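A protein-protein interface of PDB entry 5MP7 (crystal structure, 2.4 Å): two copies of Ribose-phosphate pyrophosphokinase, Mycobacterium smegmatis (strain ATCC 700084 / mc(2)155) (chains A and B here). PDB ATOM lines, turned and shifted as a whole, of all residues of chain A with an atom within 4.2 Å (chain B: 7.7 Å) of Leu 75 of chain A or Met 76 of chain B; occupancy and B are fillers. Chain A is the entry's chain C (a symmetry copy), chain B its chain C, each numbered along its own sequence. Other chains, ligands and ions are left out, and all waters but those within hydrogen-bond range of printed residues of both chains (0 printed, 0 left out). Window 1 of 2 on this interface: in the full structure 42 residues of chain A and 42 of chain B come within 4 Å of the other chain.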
ATOM      1  N   HIS A  67     -37.253  -9.501   7.015  1.00  0.00           N
ATOM      2  CA  HIS A  67     -36.315  -8.415   7.258  1.00  0.00           C
ATOM      3  C   HIS A  67     -36.734  -7.117   6.579  1.00  0.00           C
ATOM      4  O   HIS A  67     -35.997  -6.562   5.770  1.00  0.00           O
ATOM      5  CB  HIS A  67     -34.908  -8.814   6.821  1.00  0.00           C
ATOM      6  CG  HIS A  67     -34.313  -9.886   7.674  1.00  0.00           C
ATOM      7  ND1 HIS A  67     -34.489 -11.224   7.403  1.00  0.00           N
ATOM      8  CD2 HIS A  67     -33.622  -9.835   8.835  1.00  0.00           C
ATOM      9  CE1 HIS A  67     -33.930 -11.955   8.351  1.00  0.00           C
ATOM     10  NE2 HIS A  67     -33.396 -11.134   9.234  1.00  0.00           N
ATOM     11  N   LEU A  71     -33.866  -3.067   9.272  1.00  0.00           N
ATOM     12  CA  LEU A  71     -33.474  -4.440   8.964  1.00  0.00           C
ATOM     13  C   LEU A  71     -32.453  -5.085   9.924  1.00  0.00           C
ATOM     14  O   LEU A  71     -32.534  -6.286  10.213  1.00  0.00           O
ATOM     15  CB  LEU A  71     -32.976  -4.441   7.520  1.00  0.00           C
ATOM     16  CG  LEU A  71     -32.197  -5.553   6.905  1.00  0.00           C
ATOM     17  CD1 LEU A  71     -32.496  -5.611   5.404  1.00  0.00           C
ATOM     18  CD2 LEU A  71     -30.724  -5.363   7.121  1.00  0.00           C
ATOM     19  N   ASN A  72     -31.509  -4.297  10.427  1.00  0.00           N
ATOM     20  CA  ASN A  72     -30.429  -4.819  11.257  1.00  0.00           C
ATOM     21  C   ASN A  72     -30.903  -5.332  12.599  1.00  0.00           C
ATOM     22  O   ASN A  72     -30.363  -6.315  13.134  1.00  0.00           O
ATOM     23  CB  ASN A  72     -29.380  -3.764  11.432  1.00  0.00           C
ATOM     24  CG  ASN A  72     -28.821  -3.335  10.099  1.00  0.00           C
ATOM     25  OD1 ASN A  72     -28.223  -4.147   9.365  1.00  0.00           O
ATOM     26  ND2 ASN A  72     -29.034  -2.076   9.744  1.00  0.00           N
ATOM     27  N   GLN A  73     -31.917  -4.677  13.138  1.00  0.00           N
ATOM     28  CA  GLN A  73     -32.589  -5.176  14.307  1.00  0.00           C
ATOM     29  C   GLN A  73     -33.141  -6.592  14.122  1.00  0.00           C
ATOM     30  O   GLN A  73     -33.087  -7.428  15.041  1.00  0.00           O
ATOM     31  CB  GLN A  73     -33.743  -4.238  14.641  1.00  0.00           C
ATOM     32  CG  GLN A  73     -34.466  -4.546  15.935  1.00  0.00           C
ATOM     33  CD  GLN A  73     -35.680  -3.652  16.121  1.00  0.00           C
ATOM     34  OE1 GLN A  73     -35.835  -2.639  15.430  1.00  0.00           O
ATOM     35  NE2 GLN A  73     -36.580  -4.054  17.026  1.00  0.00           N
ATOM     36  N   TRP A  74     -33.779  -6.849  12.985  1.00  0.00           N
ATOM     37  CA  TRP A  74     -34.423  -8.161  12.812  1.00  0.00           C
ATOM     38  C   TRP A  74     -33.395  -9.247  12.545  1.00  0.00           C
ATOM     39  O   TRP A  74     -33.615 -10.409  12.866  1.00  0.00           O
ATOM     40  CB  TRP A  74     -35.442  -8.120  11.698  1.00  0.00           C
ATOM     41  CG  TRP A  74     -36.460  -7.057  11.868  1.00  0.00           C
ATOM     42  CD1 TRP A  74     -36.761  -6.109  10.970  1.00  0.00           C
ATOM     43  CD2 TRP A  74     -37.318  -6.849  12.991  1.00  0.00           C
ATOM     44  NE1 TRP A  74     -37.774  -5.318  11.443  1.00  0.00           N
ATOM     45  CE2 TRP A  74     -38.153  -5.766  12.671  1.00  0.00           C
ATOM     46  CE3 TRP A  74     -37.497  -7.513  14.202  1.00  0.00           C
ATOM     47  CZ2 TRP A  74     -39.127  -5.287  13.523  1.00  0.00           C
ATOM     48  CZ3 TRP A  74     -38.486  -7.046  15.070  1.00  0.00           C
ATOM     49  CH2 TRP A  74     -39.280  -5.928  14.725  1.00  0.00           C
ATOM     50  N   LEU A  75     -32.296  -8.855  11.903  1.00  0.00           N
ATOM     51  CA  LEU A  75     -31.179  -9.750  11.680  1.00  0.00           C
ATOM     52  C   LEU A  75     -30.566 -10.177  13.031  1.00  0.00           C
ATOM     53  O   LEU A  75     -30.290 -11.381  13.239  1.00  0.00           O
ATOM     54  CB  LEU A  75     -30.152  -9.119  10.735  1.00  0.00           C
ATOM     55  CG  LEU A  75     -28.950  -9.985  10.439  1.00  0.00           C
ATOM     56  CD1 LEU A  75     -29.338 -11.352   9.822  1.00  0.00           C
ATOM     57  CD2 LEU A  75     -28.035  -9.193   9.532  1.00  0.00           C
ATOM     58  N   MET A  76     -30.366  -9.223  13.935  1.00  0.00           N
ATOM     59  CA  MET A  76     -29.855  -9.546  15.261  1.00  0.00           C
ATOM     60  C   MET A  76     -30.836 -10.370  16.047  1.00  0.00           C
ATOM     61  O   MET A  76     -30.415 -11.276  16.742  1.00  0.00           O
ATOM     62  CB  MET A  76     -29.510  -8.309  16.056  1.00  0.00           C
ATOM     63  CG  MET A  76     -28.274  -7.593  15.554  1.00  0.00           C
ATOM     64  SD  MET A  76     -26.756  -8.561  15.496  1.00  0.00           S
ATOM     65  CE  MET A  76     -26.812  -9.363  17.129  1.00  0.00           C
ATOM     66  N   GLU A  77     -32.132 -10.110  15.911  1.00  0.00           N
ATOM     67  CA  GLU A  77     -33.104 -10.925  16.638  1.00  0.00           C
ATOM     68  C   GLU A  77     -33.030 -12.399  16.193  1.00  0.00           C
ATOM     69  O   GLU A  77     -33.088 -13.297  17.017  1.00  0.00           O
ATOM     70  CB  GLU A  77     -34.517 -10.387  16.480  1.00  0.00           C
ATOM     71  CG  GLU A  77     -35.587 -11.245  17.162  1.00  0.00           C
ATOM     72  CD  GLU A  77     -36.974 -10.562  17.249  1.00  0.00           C
ATOM     73  OE1 GLU A  77     -37.775 -10.588  16.258  1.00  0.00           O
ATOM     74  OE2 GLU A  77     -37.277  -9.996  18.329  1.00  0.00           O
ATOM     75  N   GLN A  78     -32.888 -12.637  14.894  1.00  0.00           N
ATOM     76  CA  GLN A  78     -32.750 -13.994  14.369  1.00  0.00           C
ATOM     77  C   GLN A  78     -31.476 -14.672  14.843  1.00  0.00           C
ATOM     78  O   GLN A  78     -31.524 -15.837  15.282  1.00  0.00           O
ATOM     79  CB  GLN A  78     -32.809 -13.978  12.840  1.00  0.00           C
ATOM     80  CG  GLN A  78     -32.812 -15.351  12.228  1.00  0.00           C
ATOM     81  CD  GLN A  78     -33.290 -15.308  10.800  1.00  0.00           C
ATOM     82  OE1 GLN A  78     -32.886 -14.446  10.049  1.00  0.00           O
ATOM     83  NE2 GLN A  78     -34.153 -16.241  10.417  1.00  0.00           N
ATOM     84  N   LEU A  79     -30.337 -13.959  14.800  1.00  0.00           N
ATOM     85  CA  LEU A  79     -29.083 -14.512  15.340  1.00  0.00           C
ATOM     86  C   LEU A  79     -29.175 -14.856  16.824  1.00  0.00           C
ATOM     87  O   LEU A  79     -28.649 -15.886  17.263  1.00  0.00           O
ATOM     88  CB  LEU A  79     -27.917 -13.559  15.156  1.00  0.00           C
ATOM     89  CG  LEU A  79     -27.577 -13.272  13.718  1.00  0.00           C
ATOM     90  CD1 LEU A  79     -26.607 -12.144  13.631  1.00  0.00           C
ATOM     91  CD2 LEU A  79     -27.012 -14.480  13.039  1.00  0.00           C
ATOM     92  N   GLY B  46     -32.774   0.122   5.363  1.00  0.00           N
ATOM     93  CA  GLY B  46     -32.012  -0.010   6.613  1.00  0.00           C
ATOM     94  C   GLY B  46     -30.647  -0.675   6.374  1.00  0.00           C
ATOM     95  O   GLY B  46     -29.802  -0.649   7.247  1.00  0.00           O
ATOM     96  N   ILE B  48     -26.959  -1.133   5.396  1.00  0.00           N
ATOM     97  CA  ILE B  48     -25.856  -0.192   5.490  1.00  0.00           C
ATOM     98  C   ILE B  48     -24.910  -0.454   4.333  1.00  0.00           C
ATOM     99  O   ILE B  48     -24.577  -1.586   4.044  1.00  0.00           O
ATOM    100  CB  ILE B  48     -25.112  -0.402   6.826  1.00  0.00           C
ATOM    101  CG1 ILE B  48     -26.044  -0.102   7.982  1.00  0.00           C
ATOM    102  CG2 ILE B  48     -23.888   0.471   6.955  1.00  0.00           C
ATOM    103  CD1 ILE B  48     -25.736  -0.979   9.168  1.00  0.00           C
ATOM    104  N   VAL B  50     -21.055   0.529   2.955  1.00  0.00           N
ATOM    105  CA  VAL B  50     -19.781   0.991   3.460  1.00  0.00           C
ATOM    106  C   VAL B  50     -18.789   0.907   2.340  1.00  0.00           C
ATOM    107  O   VAL B  50     -18.701  -0.100   1.691  1.00  0.00           O
ATOM    108  CB  VAL B  50     -19.345   0.141   4.709  1.00  0.00           C
ATOM    109  CG1 VAL B  50     -17.827   0.033   4.856  1.00  0.00           C
ATOM    110  CG2 VAL B  50     -19.908   0.728   6.003  1.00  0.00           C
ATOM    111  N   GLN B  65     -16.343   2.020  17.229  1.00  0.00           N
ATOM    112  CA  GLN B  65     -17.775   2.220  17.175  1.00  0.00           C
ATOM    113  C   GLN B  65     -18.371   2.184  18.586  1.00  0.00           C
ATOM    114  O   GLN B  65     -18.224   1.205  19.323  1.00  0.00           O
ATOM    115  CB  GLN B  65     -18.421   1.125  16.307  1.00  0.00           C
ATOM    116  CG  GLN B  65     -19.933   1.232  16.127  1.00  0.00           C
ATOM    117  CD  GLN B  65     -20.325   2.310  15.128  1.00  0.00           C
ATOM    118  OE1 GLN B  65     -20.020   3.491  15.303  1.00  0.00           O
ATOM    119  NE2 GLN B  65     -20.991   1.902  14.056  1.00  0.00           N
ATOM    120  N   HIS B  67     -22.095   2.293  20.764  1.00  0.00           N
ATOM    121  CA  HIS B  67     -23.344   1.578  20.545  1.00  0.00           C
ATOM    122  C   HIS B  67     -24.501   2.163  21.346  1.00  0.00           C
ATOM    123  O   HIS B  67     -25.126   1.474  22.147  1.00  0.00           O
ATOM    124  CB  HIS B  67     -23.175   0.095  20.860  1.00  0.00           C
ATOM    125  CG  HIS B  67     -22.283  -0.610  19.892  1.00  0.00           C
ATOM    126  ND1 HIS B  67     -20.920  -0.689  20.071  1.00  0.00           N
ATOM    127  CD2 HIS B  67     -22.530  -1.192  18.697  1.00  0.00           C
ATOM    128  CE1 HIS B  67     -20.362  -1.293  19.036  1.00  0.00           C
ATOM    129  NE2 HIS B  67     -21.320  -1.608  18.186  1.00  0.00           N
ATOM    130  N   LEU B  71     -29.160   0.254  18.793  1.00  0.00           N
ATOM    131  CA  LEU B  71     -27.862  -0.393  18.969  1.00  0.00           C
ATOM    132  C   LEU B  71     -27.472  -1.434  17.900  1.00  0.00           C
ATOM    133  O   LEU B  71     -26.297  -1.540  17.526  1.00  0.00           O
ATOM    134  CB  LEU B  71     -27.858  -0.992  20.375  1.00  0.00           C
ATOM    135  CG  LEU B  71     -26.865  -1.997  20.852  1.00  0.00           C
ATOM    136  CD1 LEU B  71     -26.660  -1.827  22.360  1.00  0.00           C
ATOM    137  CD2 LEU B  71     -27.328  -3.393  20.558  1.00  0.00           C
ATOM    138  N   ASN B  72     -28.446  -2.186  17.399  1.00  0.00           N
ATOM    139  CA  ASN B  72     -28.179  -3.273  16.465  1.00  0.00           C
ATOM    140  C   ASN B  72     -27.676  -2.795  15.120  1.00  0.00           C
ATOM    141  O   ASN B  72     -26.841  -3.455  14.479  1.00  0.00           O
ATOM    142  CB  ASN B  72     -29.412  -4.108  16.304  1.00  0.00           C
ATOM    143  CG  ASN B  72     -29.848  -4.684  17.627  1.00  0.00           C
ATOM    144  OD1 ASN B  72     -29.110  -5.468  18.258  1.00  0.00           O
ATOM    145  ND2 ASN B  72     -31.023  -4.284  18.090  1.00  0.00           N
ATOM    146  N   GLN B  73     -28.173  -1.644  14.699  1.00  0.00           N
ATOM    147  CA  GLN B  73     -27.638  -0.982  13.541  1.00  0.00           C
ATOM    148  C   GLN B  73     -26.137  -0.699  13.651  1.00  0.00           C
ATOM    149  O   GLN B  73     -25.385  -0.827  12.670  1.00  0.00           O
ATOM    150  CB  GLN B  73     -28.374   0.339  13.353  1.00  0.00           C
ATOM    151  CG  GLN B  73     -28.026   1.094  12.089  1.00  0.00           C
ATOM    152  CD  GLN B  73     -28.700   2.456  12.048  1.00  0.00           C
ATOM    153  OE1 GLN B  73     -29.623   2.730  12.824  1.00  0.00           O
ATOM    154  NE2 GLN B  73     -28.202   3.338  11.175  1.00  0.00           N
ATOM    155  N   TRP B  74     -25.699  -0.204  14.804  1.00  0.00           N
ATOM    156  CA  TRP B  74     -24.285   0.188  14.918  1.00  0.00           C
ATOM    157  C   TRP B  74     -23.384  -1.029  15.035  1.00  0.00           C
ATOM    158  O   TRP B  74     -22.225  -0.990  14.641  1.00  0.00           O
ATOM    159  CB  TRP B  74     -24.073   1.111  16.094  1.00  0.00           C
ATOM    160  CG  TRP B  74     -24.946   2.307  16.071  1.00  0.00           C
ATOM    161  CD1 TRP B  74     -25.766   2.698  17.056  1.00  0.00           C
ATOM    162  CD2 TRP B  74     -25.069   3.272  15.025  1.00  0.00           C
ATOM    163  NE1 TRP B  74     -26.393   3.867  16.711  1.00  0.00           N
ATOM    164  CE2 TRP B  74     -25.963   4.255  15.478  1.00  0.00           C
ATOM    165  CE3 TRP B  74     -24.462   3.425  13.780  1.00  0.00           C
ATOM    166  CZ2 TRP B  74     -26.315   5.359  14.729  1.00  0.00           C
ATOM    167  CZ3 TRP B  74     -24.800   4.543  13.015  1.00  0.00           C
ATOM    168  CH2 TRP B  74     -25.734   5.490  13.494  1.00  0.00           C
ATOM    169  N   LEU B  75     -23.924  -2.090  15.634  1.00  0.00           N
ATOM    170  CA  LEU B  75     -23.230  -3.359  15.716  1.00  0.00           C
ATOM    171  C   LEU B  75     -23.006  -3.932  14.300  1.00  0.00           C
ATOM    172  O   LEU B  75     -21.886  -4.396  13.984  1.00  0.00           O
ATOM    173  CB  LEU B  75     -23.972  -4.330  16.639  1.00  0.00           C
ATOM    174  CG  LEU B  75     -23.317  -5.683  16.791  1.00  0.00           C
ATOM    175  CD1 LEU B  75     -21.866  -5.585  17.325  1.00  0.00           C
ATOM    176  CD2 LEU B  75     -24.200  -6.513  17.695  1.00  0.00           C
ATOM    177  N   MET B  76     -24.036  -3.894  13.461  1.00  0.00           N
ATOM    178  CA  MET B  76     -23.895  -4.351  12.083  1.00  0.00           C
ATOM    179  C   MET B  76     -22.961  -3.469  11.302  1.00  0.00           C
ATOM    180  O   MET B  76     -22.191  -3.988  10.514  1.00  0.00           O
ATOM    181  CB  MET B  76     -25.222  -4.415  11.365  1.00  0.00           C
ATOM    182  CG  MET B  76     -26.112  -5.542  11.841  1.00  0.00           C
ATOM    183  SD  MET B  76     -25.428  -7.205  11.728  1.00  0.00           S
ATOM    184  CE  MET B  76     -24.736  -7.165  10.045  1.00  0.00           C
ATOM    185  N   GLU B  77     -22.976  -2.163  11.539  1.00  0.00           N
ATOM    186  CA  GLU B  77     -22.049  -1.294  10.816  1.00  0.00           C
ATOM    187  C   GLU B  77     -20.587  -1.656  11.142  1.00  0.00           C
ATOM    188  O   GLU B  77     -19.748  -1.692  10.257  1.00  0.00           O
ATOM    189  CB  GLU B  77     -22.316   0.174  11.104  1.00  0.00           C
ATOM    190  CG  GLU B  77     -21.327   1.129  10.428  1.00  0.00           C
ATOM    191  CD  GLU B  77     -21.756   2.615  10.482  1.00  0.00           C
ATOM    192  OE1 GLU B  77     -21.525   3.322  11.517  1.00  0.00           O
ATOM    193  OE2 GLU B  77     -22.326   3.093   9.470  1.00  0.00           O
ATOM    194  N   GLN B  78     -20.295  -1.935  12.406  1.00  0.00           N
ATOM    195  CA  GLN B  78     -18.954  -2.346  12.817  1.00  0.00           C
ATOM    196  C   GLN B  78     -18.546  -3.679  12.212  1.00  0.00           C
ATOM    197  O   GLN B  78     -17.422  -3.799  11.690  1.00  0.00           O
ATOM    198  CB  GLN B  78     -18.862  -2.401  14.343  1.00  0.00           C
ATOM    199  CG  GLN B  78     -17.475  -2.683  14.848  1.00  0.00           C
ATOM    200  CD  GLN B  78     -17.340  -2.315  16.303  1.00  0.00           C
ATOM    201  OE1 GLN B  78     -18.211  -2.620  17.090  1.00  0.00           O
ATOM    202  NE2 GLN B  78     -16.246  -1.658  16.668  1.00  0.00           N
ATOM    203  N   LEU B  79     -19.447  -4.677  12.237  1.00  0.00           N
ATOM    204  CA  LEU B  79     -19.161  -5.962  11.577  1.00  0.00           C
ATOM    205  C   LEU B  79     -18.901  -5.819  10.081  1.00  0.00           C
ATOM    206  O   LEU B  79     -18.012  -6.480   9.531  1.00  0.00           O
ATOM    207  CB  LEU B  79     -20.292  -6.956  11.759  1.00  0.00           C
ATOM    208  CG  LEU B  79     -20.544  -7.350  13.190  1.00  0.00           C
ATOM    209  CD1 LEU B  79     -21.817  -8.114  13.301  1.00  0.00           C
ATOM    210  CD2 LEU B  79     -19.414  -8.166  13.737  1.00  0.00           C
ATOM    211  N   ILE B  80     -19.683  -4.966   9.412  1.00  0.00           N
ATOM    212  CA  ILE B  80     -19.526  -4.736   7.967  1.00  0.00           C
ATOM    213  C   ILE B  80     -18.182  -4.097   7.675  1.00  0.00           C
ATOM    214  O   ILE B  80     -17.513  -4.475   6.717  1.00  0.00           O
ATOM    215  CB  ILE B  80     -20.719  -3.928   7.396  1.00  0.00           C
ATOM    216  CG1 ILE B  80     -21.934  -4.840   7.306  1.00  0.00           C
ATOM    217  CG2 ILE B  80     -20.453  -3.379   6.008  1.00  0.00           C
ATOM    218  CD1 ILE B  80     -23.248  -4.087   7.280  1.00  0.00           C
ATOM    219  N   MET B  81     -17.774  -3.137   8.483  1.00  0.00           N
ATOM    220  CA  MET B  81     -16.448  -2.485   8.305  1.00  0.00           C
ATOM    221  C   MET B  81     -15.291  -3.459   8.509  1.00  0.00           C
ATOM    222  O   MET B  81     -14.305  -3.411   7.805  1.00  0.00           O
ATOM    223  CB  MET B  81     -16.285  -1.303   9.278  1.00  0.00           C
ATOM    224  CG  MET B  81     -16.991  -0.044   8.823  1.00  0.00           C
ATOM    225  SD  MET B  81     -17.182   1.271  10.066  1.00  0.00           S
ATOM    226  CE  MET B  81     -15.586   1.994   9.997  1.00  0.00           C
ATOM    227  N   ILE B  82     -15.425  -4.337   9.478  1.00  0.00           N
ATOM    228  CA  ILE B  82     -14.418  -5.352   9.713  1.00  0.00           C
ATOM    229  C   ILE B  82     -14.320  -6.353   8.548  1.00  0.00           C
ATOM    230  O   ILE B  82     -13.219  -6.691   8.155  1.00  0.00           O
ATOM    231  CB  ILE B  82     -14.674  -6.025  11.055  1.00  0.00           C
ATOM    232  CG1 ILE B  82     -14.396  -5.022  12.168  1.00  0.00           C
ATOM    233  CG2 ILE B  82     -13.802  -7.236  11.253  1.00  0.00           C
ATOM    234  CD1 ILE B  82     -15.039  -5.374  13.484  1.00  0.00           C
ATOM    235  N   LEU B 119     -22.251 -14.309  21.971  1.00  0.00           N
ATOM    236  CA  LEU B 119     -22.565 -14.209  20.527  1.00  0.00           C
ATOM    237  C   LEU B 119     -21.906 -13.022  19.876  1.00  0.00           C
ATOM    238  O   LEU B 119     -21.365 -13.157  18.802  1.00  0.00           O
ATOM    239  CB  LEU B 119     -24.073 -14.151  20.283  1.00  0.00           C
ATOM    240  CG  LEU B 119     -24.550 -14.023  18.825  1.00  0.00           C
ATOM    241  CD1 LEU B 119     -24.230 -15.284  18.028  1.00  0.00           C
ATOM    242  CD2 LEU B 119     -26.026 -13.712  18.822  1.00  0.00           C
ATOM    243  N   LEU B 123     -19.347 -13.220  16.665  1.00  0.00           N
ATOM    244  CA  LEU B 123     -19.615 -12.508  15.444  1.00  0.00           C
ATOM    245  C   LEU B 123     -18.442 -11.594  15.060  1.00  0.00           C
ATOM    246  O   LEU B 123     -18.090 -11.514  13.885  1.00  0.00           O
ATOM    247  CB  LEU B 123     -20.875 -11.680  15.568  1.00  0.00           C
ATOM    248  CG  LEU B 123     -22.177 -12.361  15.905  1.00  0.00           C
ATOM    249  CD1 LEU B 123     -23.286 -11.325  15.824  1.00  0.00           C
ATOM    250  CD2 LEU B 123     -22.505 -13.558  15.026  1.00  0.00           C
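Among the printed residues, merely in contact across the chains: Asn 72 of chain A with Ile 48 of chain B (3.5 Å), Met 76 of chain A with Asn 72 of chain B (3.5 Å), Asn 72 of chain A with Met 76 of chain B (3.5 Å), Leu 79 of chain A with Leu 119 of chain B (3.7 Å), Gln 73 of chain A with Asn 72 of chain B (3.9 Å), Asn 72 of chain A with Gln 73 of chain B (3.9 Å), Leu 75 of chain A with Met 76 of chain B (3.9 Å), Met 76 of chain A with Leu 75 of chain B (3.9 Å) and Asn 72 of chain A with Asn 72 of chain B (3.98 Å).
Printed residues of chain B within 4 Å of Leu 75 of chain A: Met 76 (3.9 Å). Met 76 of chain B touches two residues of chain A. Printed residues of chain A within 4 Å of Leu 119 of chain B: Leu 79 (3.7 Å). Of the printed residues of chain A, Gly 46 of chain B touches Asn 72 (3.0 Å). Of the printed residues of chain B, Gln 73 of chain A touches Asn 72 (3.9 Å). Of the printed residues of chain B, Leu 79 of chain A touches Leu 119. Printed residues of chain A within 4 Å of Asn 72 of chain B: Asn 72 (3.98 Å), Gln 73 (3.9 Å) and Met 76 (3.5 Å). Leu 79 of chain B touches none of the printed residues of chain A.
The backbone carbonyl oxygen of Gly 46 of chain B lies within hydrogen-bond range of the side-chain amide nitrogen of Asn 72 of chain A, 3.0 Å away.
Asn 72 of chain A touches its own counterpart, Asn 72 of chain B. Asn 72 of chain A touches Gln 73 of chain B, and with the chains exchanged Gln 73 of chain A touches Asn 72 of chain B. Asn 72 of chain A touches Met 76 of chain B, and with the chains exchanged Met 76 of chain A touches Asn 72 of chain B. Leu 75 of chain A touches Met 76 of chain B, and with the chains exchanged Met 76 of chain A touches Leu 75 of chain B.
Of the 19 printed residues of chain B, 7 touch a printed residue of chain A. Hydrophobic or aromatic side chains of chain B that line the printed part of chain A: Ile 48, Leu 75, Met 76 and Leu 119. Among the printed residues, no Asp or Glu carboxylate lies within 4 Å of a Lys or Arg side-chain nitrogen of the other chain.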
